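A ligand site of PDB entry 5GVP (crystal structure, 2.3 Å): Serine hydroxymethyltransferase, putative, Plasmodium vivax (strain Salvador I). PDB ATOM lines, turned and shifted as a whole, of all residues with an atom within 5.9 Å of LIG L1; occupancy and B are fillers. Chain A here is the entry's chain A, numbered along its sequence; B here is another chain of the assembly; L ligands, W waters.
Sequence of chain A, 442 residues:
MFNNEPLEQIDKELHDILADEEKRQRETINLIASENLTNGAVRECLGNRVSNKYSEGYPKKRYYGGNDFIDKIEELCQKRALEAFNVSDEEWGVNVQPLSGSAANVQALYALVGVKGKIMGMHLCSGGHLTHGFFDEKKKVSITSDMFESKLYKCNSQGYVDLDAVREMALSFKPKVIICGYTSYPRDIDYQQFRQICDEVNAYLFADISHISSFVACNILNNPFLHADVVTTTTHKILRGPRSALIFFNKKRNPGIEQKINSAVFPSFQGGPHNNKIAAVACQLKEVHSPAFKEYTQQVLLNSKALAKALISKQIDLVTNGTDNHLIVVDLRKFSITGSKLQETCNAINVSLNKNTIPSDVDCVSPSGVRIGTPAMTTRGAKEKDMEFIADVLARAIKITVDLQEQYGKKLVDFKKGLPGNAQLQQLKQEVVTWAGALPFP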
ATOM      1  N   HIS A 123     -20.464  10.689  -6.134  1.00  0.00           N
ATOM      2  CA  HIS A 123     -20.193  12.049  -6.597  1.00  0.00           C
ATOM      3  C   HIS A 123     -18.718  12.177  -7.039  1.00  0.00           C
ATOM      4  O   HIS A 123     -17.824  11.554  -6.452  1.00  0.00           O
ATOM      5  CB  HIS A 123     -20.533  13.017  -5.471  1.00  0.00           C
ATOM      6  CG  HIS A 123     -20.677  14.426  -5.923  1.00  0.00           C
ATOM      7  ND1 HIS A 123     -19.586  15.220  -6.215  1.00  0.00           N
ATOM      8  CD2 HIS A 123     -21.774  15.190  -6.133  1.00  0.00           C
ATOM      9  CE1 HIS A 123     -20.015  16.407  -6.606  1.00  0.00           C
ATOM     10  NE2 HIS A 123     -21.336  16.412  -6.564  1.00  0.00           N
ATOM     11  N   LEU A 124     -18.468  12.965  -8.092  1.00  0.00           N
ATOM     12  CA  LEU A 124     -17.094  13.189  -8.612  1.00  0.00           C
ATOM     13  C   LEU A 124     -16.130  13.625  -7.525  1.00  0.00           C
ATOM     14  O   LEU A 124     -15.077  13.014  -7.333  1.00  0.00           O
ATOM     15  CB  LEU A 124     -17.100  14.244  -9.741  1.00  0.00           C
ATOM     16  CG  LEU A 124     -15.755  14.743 -10.342  1.00  0.00           C
ATOM     17  CD1 LEU A 124     -15.192  13.744 -11.330  1.00  0.00           C
ATOM     18  CD2 LEU A 124     -15.930  16.100 -11.020  1.00  0.00           C
ATOM     19  N   CYS A 125     -16.490  14.724  -6.863  1.00  0.00           N
ATOM     20  CA  CYS A 125     -15.790  15.270  -5.682  1.00  0.00           C
ATOM     21  C   CYS A 125     -15.554  14.287  -4.504  1.00  0.00           C
ATOM     22  O   CYS A 125     -14.658  14.520  -3.707  1.00  0.00           O
ATOM     23  CB  CYS A 125     -16.504  16.544  -5.191  1.00  0.00           C
ATOM     24  SG  CYS A 125     -16.823  17.773  -6.503  1.00  0.00           S
ATOM     25  N   SER A 126     -16.347  13.233  -4.402  1.00  0.00           N
ATOM     26  CA  SER A 126     -16.134  12.184  -3.398  1.00  0.00           C
ATOM     27  C   SER A 126     -15.399  10.949  -3.921  1.00  0.00           C
ATOM     28  O   SER A 126     -15.248   9.976  -3.193  1.00  0.00           O
ATOM     29  CB  SER A 126     -17.486  11.777  -2.807  1.00  0.00           C
ATOM     30  OG  SER A 126     -18.179  12.903  -2.302  1.00  0.00           O
ATOM     31  N   GLY A 127     -14.941  10.978  -5.164  1.00  0.00           N
ATOM     32  CA  GLY A 127     -14.123   9.896  -5.723  1.00  0.00           C
ATOM     33  C   GLY A 127     -14.756   9.086  -6.846  1.00  0.00           C
ATOM     34  O   GLY A 127     -14.112   8.207  -7.370  1.00  0.00           O
ATOM     35  N   GLY A 128     -15.994   9.398  -7.237  1.00  0.00           N
ATOM     36  CA  GLY A 128     -16.616   8.710  -8.359  1.00  0.00           C
ATOM     37  C   GLY A 128     -16.144   9.263  -9.688  1.00  0.00           C
ATOM     38  O   GLY A 128     -15.574  10.364  -9.752  1.00  0.00           O
ATOM     39  N   HIS A 129     -16.329   8.484 -10.768  1.00  0.00           N
ATOM     40  CA  HIS A 129     -16.019   8.956 -12.112  1.00  0.00           C
ATOM     41  C   HIS A 129     -17.091   9.879 -12.687  1.00  0.00           C
ATOM     42  O   HIS A 129     -18.231   9.916 -12.251  1.00  0.00           O
ATOM     43  CB  HIS A 129     -15.759   7.761 -13.058  1.00  0.00           C
ATOM     44  CG  HIS A 129     -14.976   8.137 -14.286  1.00  0.00           C
ATOM     45  ND1 HIS A 129     -15.494   8.023 -15.547  1.00  0.00           N
ATOM     46  CD2 HIS A 129     -13.736   8.666 -14.439  1.00  0.00           C
ATOM     47  CE1 HIS A 129     -14.611   8.459 -16.435  1.00  0.00           C
ATOM     48  NE2 HIS A 129     -13.529   8.846 -15.776  1.00  0.00           N
ATOM     49  N   LEU A 130     -16.657  10.640 -13.685  1.00  0.00           N
ATOM     50  CA  LEU A 130     -17.548  11.466 -14.512  1.00  0.00           C
ATOM     51  C   LEU A 130     -18.698  10.642 -15.081  1.00  0.00           C
ATOM     52  O   LEU A 130     -19.867  11.047 -14.990  1.00  0.00           O
ATOM     53  CB  LEU A 130     -16.735  12.067 -15.663  1.00  0.00           C
ATOM     54  CG  LEU A 130     -15.611  13.027 -15.252  1.00  0.00           C
ATOM     55  CD1 LEU A 130     -14.631  13.245 -16.390  1.00  0.00           C
ATOM     56  CD2 LEU A 130     -16.201  14.354 -14.794  1.00  0.00           C
ATOM     57  N   PHE A 134     -22.104  12.205 -13.213  1.00  0.00           N
ATOM     58  CA  PHE A 134     -21.681  13.483 -12.690  1.00  0.00           C
ATOM     59  C   PHE A 134     -22.387  14.664 -13.325  1.00  0.00           C
ATOM     60  O   PHE A 134     -22.330  14.838 -14.543  1.00  0.00           O
ATOM     61  CB  PHE A 134     -20.185  13.708 -12.889  1.00  0.00           C
ATOM     62  CG  PHE A 134     -19.741  15.038 -12.401  1.00  0.00           C
ATOM     63  CD1 PHE A 134     -19.888  15.367 -11.045  1.00  0.00           C
ATOM     64  CD2 PHE A 134     -19.249  15.987 -13.273  1.00  0.00           C
ATOM     65  CE1 PHE A 134     -19.526  16.609 -10.573  1.00  0.00           C
ATOM     66  CE2 PHE A 134     -18.886  17.229 -12.801  1.00  0.00           C
ATOM     67  CZ  PHE A 134     -19.007  17.544 -11.452  1.00  0.00           C
ATOM     68  N   VAL A 141     -22.763  17.802 -16.749  1.00  0.00           N
ATOM     69  CA  VAL A 141     -21.385  17.788 -17.227  1.00  0.00           C
ATOM     70  C   VAL A 141     -21.070  16.496 -17.998  1.00  0.00           C
ATOM     71  O   VAL A 141     -20.342  16.525 -18.995  1.00  0.00           O
ATOM     72  CB  VAL A 141     -20.418  17.948 -16.021  1.00  0.00           C
ATOM     73  CG1 VAL A 141     -18.955  17.754 -16.416  1.00  0.00           C
ATOM     74  CG2 VAL A 141     -20.621  19.305 -15.355  1.00  0.00           C
ATOM     75  N   THR A 183     -12.800   6.404  -8.912  1.00  0.00           N
ATOM     76  CA  THR A 183     -11.552   6.922  -9.519  1.00  0.00           C
ATOM     77  C   THR A 183     -10.501   7.281  -8.479  1.00  0.00           C
ATOM     78  O   THR A 183      -9.334   6.975  -8.687  1.00  0.00           O
ATOM     79  CB  THR A 183     -11.718   8.075 -10.550  1.00  0.00           C
ATOM     80  OG1 THR A 183     -11.224   9.328 -10.056  1.00  0.00           O
ATOM     81  CG2 THR A 183     -13.121   8.213 -11.006  1.00  0.00           C
ATOM     82  N   SER A 184     -10.914   7.864  -7.353  1.00  0.00           N
ATOM     83  CA  SER A 184      -9.989   8.263  -6.271  1.00  0.00           C
ATOM     84  C   SER A 184     -10.511   7.822  -4.901  1.00  0.00           C
ATOM     85  O   SER A 184     -10.720   8.631  -4.012  1.00  0.00           O
ATOM     86  CB  SER A 184      -9.757   9.786  -6.303  1.00  0.00           C
ATOM     87  OG  SER A 184      -9.940  10.325  -7.604  1.00  0.00           O
ATOM     88  N   ASN A 354      -1.720  14.286  -9.556  1.00  0.00           N
ATOM     89  CA  ASN A 354      -2.858  15.133  -9.839  1.00  0.00           C
ATOM     90  C   ASN A 354      -3.499  15.679  -8.609  1.00  0.00           C
ATOM     91  O   ASN A 354      -3.445  15.093  -7.547  1.00  0.00           O
ATOM     92  CB  ASN A 354      -3.891  14.470 -10.759  1.00  0.00           C
ATOM     93  CG  ASN A 354      -4.609  13.311 -10.107  1.00  0.00           C
ATOM     94  OD1 ASN A 354      -4.168  12.180 -10.210  1.00  0.00           O
ATOM     95  ND2 ASN A 354      -5.695  13.597  -9.414  1.00  0.00           N
ATOM     96  N   LYS A 355      -4.068  16.856  -8.799  1.00  0.00           N
ATOM     97  CA  LYS A 355      -4.887  17.503  -7.814  1.00  0.00           C
ATOM     98  C   LYS A 355      -6.165  16.727  -7.637  1.00  0.00           C
ATOM     99  O   LYS A 355      -6.674  16.106  -8.581  1.00  0.00           O
ATOM    100  CB  LYS A 355      -5.191  18.960  -8.215  1.00  0.00           C
ATOM    101  CG  LYS A 355      -5.603  19.183  -9.680  1.00  0.00           C
ATOM    102  CD  LYS A 355      -6.432  20.442  -9.836  1.00  0.00           C
ATOM    103  CE  LYS A 355      -6.420  20.922 -11.271  1.00  0.00           C
ATOM    104  NZ  LYS A 355      -7.498  21.924 -11.466  1.00  0.00           N
ATOM    105  N   ASN A 356      -6.716  16.765  -6.418  1.00  0.00           N
ATOM    106  CA  ASN A 356      -7.823  15.895  -6.100  1.00  0.00           C
ATOM    107  C   ASN A 356      -8.631  16.431  -4.935  1.00  0.00           C
ATOM    108  O   ASN A 356      -8.077  16.862  -3.916  1.00  0.00           O
ATOM    109  CB  ASN A 356      -7.305  14.486  -5.779  1.00  0.00           C
ATOM    110  CG  ASN A 356      -8.340  13.399  -6.073  1.00  0.00           C
ATOM    111  OD1 ASN A 356      -8.262  12.679  -7.092  1.00  0.00           O
ATOM    112  ND2 ASN A 356      -9.337  13.302  -5.208  1.00  0.00           N
ATOM    113  N   THR A 357      -9.941  16.362  -5.075  1.00  0.00           N
ATOM    114  CA  THR A 357     -10.843  16.765  -3.990  1.00  0.00           C
ATOM    115  C   THR A 357     -10.639  15.920  -2.738  1.00  0.00           C
ATOM    116  O   THR A 357     -10.039  14.848  -2.781  1.00  0.00           O
ATOM    117  CB  THR A 357     -12.296  16.605  -4.433  1.00  0.00           C
ATOM    118  OG1 THR A 357     -12.474  15.284  -4.970  1.00  0.00           O
ATOM    119  CG2 THR A 357     -12.632  17.659  -5.506  1.00  0.00           C
ATOM    120  N   CYS A 364     -16.022  21.700  -5.765  1.00  0.00           N
ATOM    121  CA  CYS A 364     -14.860  21.248  -6.531  1.00  0.00           C
ATOM    122  C   CYS A 364     -13.902  22.383  -6.988  1.00  0.00           C
ATOM    123  O   CYS A 364     -12.884  22.100  -7.661  1.00  0.00           O
ATOM    124  CB  CYS A 364     -15.320  20.480  -7.774  1.00  0.00           C
ATOM    125  SG  CYS A 364     -14.149  19.234  -8.341  1.00  0.00           S
ATOM    126  N   VAL A 365     -14.201  23.641  -6.638  1.00  0.00           N
ATOM    127  CA  VAL A 365     -13.517  24.838  -7.212  1.00  0.00           C
ATOM    128  C   VAL A 365     -12.026  24.849  -6.823  1.00  0.00           C
ATOM    129  O   VAL A 365     -11.159  25.126  -7.674  1.00  0.00           O
ATOM    130  CB  VAL A 365     -14.212  26.182  -6.789  1.00  0.00           C
ATOM    131  CG1 VAL A 365     -13.437  27.398  -7.276  1.00  0.00           C
ATOM    132  CG2 VAL A 365     -15.657  26.247  -7.306  1.00  0.00           C
ATOM    133  N   PRO A 367      -9.671  21.994  -5.062  1.00  0.00           N
ATOM    134  CA  PRO A 367      -9.331  20.738  -4.384  1.00  0.00           C
ATOM    135  C   PRO A 367      -8.192  20.907  -3.376  1.00  0.00           C
ATOM    136  O   PRO A 367      -7.132  21.445  -3.719  1.00  0.00           O
ATOM    137  CB  PRO A 367      -8.876  19.838  -5.532  1.00  0.00           C
ATOM    138  CG  PRO A 367      -8.327  20.792  -6.538  1.00  0.00           C
ATOM    139  CD  PRO A 367      -9.283  21.942  -6.484  1.00  0.00           C
ATOM    140  N   ARG A 371      -3.775  13.260  -5.331  1.00  0.00           N
ATOM    141  CA  ARG A 371      -3.894  11.855  -5.380  1.00  0.00           C
ATOM    142  C   ARG A 371      -2.601  11.349  -5.967  1.00  0.00           C
ATOM    143  O   ARG A 371      -2.050  11.976  -6.908  1.00  0.00           O
ATOM    144  CB  ARG A 371      -5.105  11.484  -6.234  1.00  0.00           C
ATOM    145  CG  ARG A 371      -5.328  10.006  -6.452  1.00  0.00           C
ATOM    146  CD  ARG A 371      -6.323   9.752  -7.565  1.00  0.00           C
ATOM    147  NE  ARG A 371      -5.741   9.994  -8.884  1.00  0.00           N
ATOM    148  CZ  ARG A 371      -6.257   9.560 -10.029  1.00  0.00           C
ATOM    149  NH1 ARG A 371      -7.392   8.838 -10.048  1.00  0.00           N
ATOM    150  NH2 ARG A 371      -5.618   9.817 -11.177  1.00  0.00           N
ATOM    151  N   GLU B  56      -6.485  14.352 -19.944  1.00  0.00           N
ATOM    152  CA  GLU B  56      -7.853  14.841 -20.016  1.00  0.00           C
ATOM    153  C   GLU B  56      -7.962  16.351 -20.082  1.00  0.00           C
ATOM    154  O   GLU B  56      -7.349  17.051 -19.296  1.00  0.00           O
ATOM    155  CB  GLU B  56      -8.640  14.392 -18.798  1.00  0.00           C
ATOM    156  CG  GLU B  56      -8.905  12.902 -18.729  1.00  0.00           C
ATOM    157  CD  GLU B  56      -9.522  12.517 -17.412  1.00  0.00           C
ATOM    158  OE1 GLU B  56      -8.757  12.314 -16.454  1.00  0.00           O
ATOM    159  OE2 GLU B  56     -10.753  12.474 -17.306  1.00  0.00           O
ATOM    160  N   TYR B  63      -6.053  18.745 -17.184  1.00  0.00           N
ATOM    161  CA  TYR B  63      -6.286  18.489 -15.777  1.00  0.00           C
ATOM    162  C   TYR B  63      -4.989  18.151 -15.105  1.00  0.00           C
ATOM    163  O   TYR B  63      -4.772  18.595 -13.978  1.00  0.00           O
ATOM    164  CB  TYR B  63      -7.422  17.462 -15.513  1.00  0.00           C
ATOM    165  CG  TYR B  63      -8.750  18.176 -15.449  1.00  0.00           C
ATOM    166  CD1 TYR B  63      -9.469  18.411 -16.603  1.00  0.00           C
ATOM    167  CD2 TYR B  63      -9.221  18.709 -14.267  1.00  0.00           C
ATOM    168  CE1 TYR B  63     -10.668  19.114 -16.575  1.00  0.00           C
ATOM    169  CE2 TYR B  63     -10.411  19.434 -14.234  1.00  0.00           C
ATOM    170  CZ  TYR B  63     -11.123  19.633 -15.386  1.00  0.00           C
ATOM    171  OH  TYR B  63     -12.310  20.325 -15.392  1.00  0.00           O
ATOM    172  N   TYR B  64      -4.109  17.404 -15.768  1.00  0.00           N
ATOM    173  CA  TYR B  64      -2.759  17.148 -15.228  1.00  0.00           C
ATOM    174  C   TYR B  64      -1.692  17.963 -15.906  1.00  0.00           C
ATOM    175  O   TYR B  64      -1.894  18.495 -16.990  1.00  0.00           O
ATOM    176  CB  TYR B  64      -2.373  15.679 -15.354  1.00  0.00           C
ATOM    177  CG  TYR B  64      -3.429  14.717 -14.924  1.00  0.00           C
ATOM    178  CD1 TYR B  64      -4.434  15.103 -14.016  1.00  0.00           C
ATOM    179  CD2 TYR B  64      -3.424  13.420 -15.392  1.00  0.00           C
ATOM    180  CE1 TYR B  64      -5.405  14.200 -13.629  1.00  0.00           C
ATOM    181  CE2 TYR B  64      -4.394  12.518 -15.004  1.00  0.00           C
ATOM    182  CZ  TYR B  64      -5.378  12.900 -14.124  1.00  0.00           C
ATOM    183  OH  TYR B  64      -6.338  12.010 -13.752  1.00  0.00           O
ATOM    184  N   PHE B 266     -15.121  16.075 -24.576  1.00  0.00           N
ATOM    185  CA  PHE B 266     -14.731  15.909 -23.165  1.00  0.00           C
ATOM    186  C   PHE B 266     -15.253  17.083 -22.360  1.00  0.00           C
ATOM    187  O   PHE B 266     -15.113  18.214 -22.764  1.00  0.00           O
ATOM    188  CB  PHE B 266     -13.219  15.804 -22.998  1.00  0.00           C
ATOM    189  CG  PHE B 266     -12.774  15.878 -21.552  1.00  0.00           C
ATOM    190  CD1 PHE B 266     -12.752  14.721 -20.761  1.00  0.00           C
ATOM    191  CD2 PHE B 266     -12.383  17.091 -20.979  1.00  0.00           C
ATOM    192  CE1 PHE B 266     -12.350  14.771 -19.436  1.00  0.00           C
ATOM    193  CE2 PHE B 266     -11.972  17.149 -19.647  1.00  0.00           C
ATOM    194  CZ  PHE B 266     -11.958  15.988 -18.885  1.00  0.00           C
ATOM    195  N   PRO B 267     -15.848  16.837 -21.184  1.00  0.00           N
ATOM    196  CA  PRO B 267     -16.057  15.597 -20.471  1.00  0.00           C
ATOM    197  C   PRO B 267     -17.466  14.996 -20.636  1.00  0.00           C
ATOM    198  O   PRO B 267     -17.825  14.129 -19.846  1.00  0.00           O
ATOM    199  CB  PRO B 267     -15.844  16.033 -19.026  1.00  0.00           C
ATOM    200  CG  PRO B 267     -16.477  17.381 -19.000  1.00  0.00           C
ATOM    201  CD  PRO B 267     -16.297  17.983 -20.375  1.00  0.00           C
HETATM  202  O1  LIG L   1     -14.738  23.416 -13.504  1.00  0.00           O
HETATM  203  C1  LIG L   1     -15.615  22.563 -13.813  1.00  0.00           C
HETATM  204  O2  LIG L   1     -16.332  22.671 -14.846  1.00  0.00           O
HETATM  205  C2  LIG L   1     -15.788  21.382 -12.878  1.00  0.00           C
HETATM  206  C3  LIG L   1     -16.380  20.114 -13.531  1.00  0.00           C
HETATM  207  C4  LIG L   1     -15.297  19.151 -13.952  1.00  0.00           C
HETATM  208  C5  LIG L   1     -14.417  18.669 -13.001  1.00  0.00           C
HETATM  209  C6  LIG L   1     -15.200  18.741 -15.271  1.00  0.00           C
HETATM  210  C7  LIG L   1     -14.210  17.848 -15.643  1.00  0.00           C
HETATM  211  C8  LIG L   1     -13.321  17.374 -14.685  1.00  0.00           C
HETATM  212  C9  LIG L   1     -13.425  17.778 -13.363  1.00  0.00           C
HETATM  213  C10 LIG L   1     -12.464  17.268 -12.358  1.00  0.00           C
HETATM  214  C11 LIG L   1     -11.872  18.158 -11.486  1.00  0.00           C
HETATM  215  C12 LIG L   1     -10.951  17.703 -10.550  1.00  0.00           C
HETATM  216  C13 LIG L   1     -10.295  18.697  -9.596  1.00  0.00           C
HETATM  217  F1  LIG L   1      -9.454  18.162  -8.720  1.00  0.00           F
HETATM  218  F2  LIG L   1      -9.655  19.621 -10.288  1.00  0.00           F
HETATM  219  F3  LIG L   1     -11.267  19.301  -8.928  1.00  0.00           F
HETATM  220  C14 LIG L   1     -10.630  16.351 -10.484  1.00  0.00           C
HETATM  221  C15 LIG L   1     -12.173  15.902 -12.291  1.00  0.00           C
HETATM  222  C16 LIG L   1     -11.228  15.403 -11.368  1.00  0.00           C
HETATM  223  C17 LIG L   1     -10.910  13.919 -11.272  1.00  0.00           C
HETATM  224  C18 LIG L   1      -9.421  13.592 -10.953  1.00  0.00           C
HETATM  225  C19 LIG L   1      -9.083  12.094 -10.913  1.00  0.00           C
HETATM  226  C20 LIG L   1      -8.389  14.296 -11.867  1.00  0.00           C
HETATM  227  C21 LIG L   1     -11.735  13.372 -10.093  1.00  0.00           C
HETATM  228  C22 LIG L   1     -11.629  13.991  -8.988  1.00  0.00           C
HETATM  229  N1  LIG L   1     -11.537  14.568  -7.978  1.00  0.00           N
HETATM  230  C23 LIG L   1     -12.497  12.251 -10.179  1.00  0.00           C
HETATM  231  N2  LIG L   1     -13.195  11.738  -9.178  1.00  0.00           N
HETATM  232  C24 LIG L   1     -11.273  13.206 -12.540  1.00  0.00           C
HETATM  233  C25 LIG L   1     -10.958  13.408 -13.986  1.00  0.00           C
HETATM  234  C26 LIG L   1     -10.108  14.468 -14.632  1.00  0.00           C
HETATM  235  N3  LIG L   1     -11.614  12.425 -14.637  1.00  0.00           N
HETATM  236  N4  LIG L   1     -12.372  11.562 -13.803  1.00  0.00           N
HETATM  237  C27 LIG L   1     -12.141  12.033 -12.578  1.00  0.00           C
HETATM  238  O3  LIG L   1     -12.638  11.522 -11.416  1.00  0.00           O
HETATM  239  N1  LG2 L   2     -13.842   4.553 -14.894  1.00  0.00           N
HETATM  240  C1  LG2 L   2     -13.089   4.890 -13.837  1.00  0.00           C
HETATM  241  C2  LG2 L   2     -13.416   4.357 -12.470  1.00  0.00           C
HETATM  242  C3  LG2 L   2     -11.930   5.795 -14.060  1.00  0.00           C
HETATM  243  O1  LG2 L   2     -11.149   6.164 -13.036  1.00  0.00           O
HETATM  244  C4  LG2 L   2     -11.653   6.293 -15.418  1.00  0.00           C
HETATM  245  C5  LG2 L   2     -10.473   7.222 -15.671  1.00  0.00           C
HETATM  246  C6  LG2 L   2     -12.584   5.817 -16.488  1.00  0.00           C
HETATM  247  C7  LG2 L   2     -13.650   4.981 -16.133  1.00  0.00           C
HETATM  248  C8  LG2 L   2     -12.511   6.246 -17.934  1.00  0.00           C
HETATM  249  O2  LG2 L   2     -11.423   5.733 -18.669  1.00  0.00           O
HETATM  250  P1  LG2 L   2     -11.065   6.401 -20.095  1.00  0.00           P
HETATM  251  O3  LG2 L   2     -12.356   6.861 -20.712  1.00  0.00           O
HETATM  252  O4  LG2 L   2     -10.209   7.570 -19.717  1.00  0.00           O
HETATM  253  O5  LG2 L   2     -10.269   5.290 -20.706  1.00  0.00           O
HETATM  254  C9  LG2 L   2      -7.952   8.868 -13.651  1.00  0.00           C
HETATM  255  O6  LG2 L   2      -6.848   9.367 -13.813  1.00  0.00           O
HETATM  256  O7  LG2 L   2      -8.190   8.219 -12.621  1.00  0.00           O
HETATM  257  C10 LG2 L   2      -9.005   9.054 -14.732  1.00  0.00           C
HETATM  258  N2  LG2 L   2     -10.141   8.157 -14.612  1.00  0.00           N
HETATM  259  O   HOH W   1     -16.153  21.201 -17.382  1.00  0.00           O
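A fluorine (F2) of LIG L1 sits close to the side-chain amino group of Lys 355.
A fluorine (F3) of LIG L1 lies close to the side-chain sulfur of Cys 364 (2.9 Å).
Residues that only touch LIG L1: Gly 127 (3.9 Å), His 129 (3.3 Å), Leu 130 (3.6 Å), Phe 134 (3.9 Å), Ser 184 (3.8 Å), Asn 354 (3.7 Å), Asn 356 (3.8 Å), Pro 367 (3.6 Å), Arg 371 (3.8 Å), Tyr 63 of chain B (3.1 Å) and Tyr 64 of chain B (3.5 Å).
Hydrophobic or aromatic side chains that line LIG L1: Leu 124, His 129, Leu 130, Phe 134, Pro 367, Tyr 63 of chain B and Tyr 64 of chain B.
18 residues have an atom within 4 Å of LIG L1: Leu 124, Gly 127, Gly 128, His 129, Leu 130, Phe 134, Thr 183, Ser 184, Asn 354, Lys 355, Asn 356, Thr 357, Cys 364, Pro 367, Arg 371, Glu 56 of chain B, Tyr 63 of chain B and Tyr 64 of chain B.
The nearest printed residue that does not touch LIG L1 is Val 141 (4.05 Å).
The backbone carbonyl oxygen (O) of Leu 124 lies within hydrogen-bond range of a nitrogen (N2) of LIG L1.
OG1 of Thr 183 lies within hydrogen-bond range of O3 of LIG L1 (2.9 Å).
An oxygen (O7) of LG2 L2 lies within salt-bridge range of the guanidinium group of Arg 371.
A nitrogen (N1) of LIG L1 is in hydrogen-bond range of the side-chain hydroxyl (OG1) of Thr 357, 3.2 Å away.
The side-chain carboxylate (OE2) of Glu 56 of chain B lies within hydrogen-bond range of a nitrogen (N3) of LIG L1 (2.8 Å).
The backbone carbonyl oxygen of Gly 128 lies within hydrogen-bond range of a nitrogen (N2) of LIG L1, at 2.8 Å.
The side-chain hydroxyl (OH) of Tyr 64 of chain B lies within hydrogen-bond range of an oxygen (O6) of LG2 L2, at 2.7 Å.
The backbone NH (N) of Ser 184 is in hydrogen-bond range of the backbone carbonyl oxygen (O) of Gly 127 (3.2 Å).
O of Thr 183 is in hydrogen-bond range of NH1 of Arg 371, 3.0 Å away.
The side-chain hydroxyl of Thr 357 is in hydrogen-bond range of the backbone carbonyl oxygen of Cys 125.
O of Glu 56 of chain B sits at hydrogen-bond distance from N of Tyr 63 of chain B (3.0 Å).
The side-chain sulfur (SG) of Cys 125 sits close to the side-chain sulfur (SG) of Cys 364, at 3.6 Å.
OG of Ser 184 is in hydrogen-bond range of OD1 of Asn 356, at 2.9 Å.
The backbone carbonyl oxygen of Asn 354 lies within hydrogen-bond range of the backbone NH of Arg 371 (2.9 Å).
The backbone carbonyl oxygen (O) of Gly 127 is in hydrogen-bond range of the backbone NH (N) of Thr 183, at 2.7 Å.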
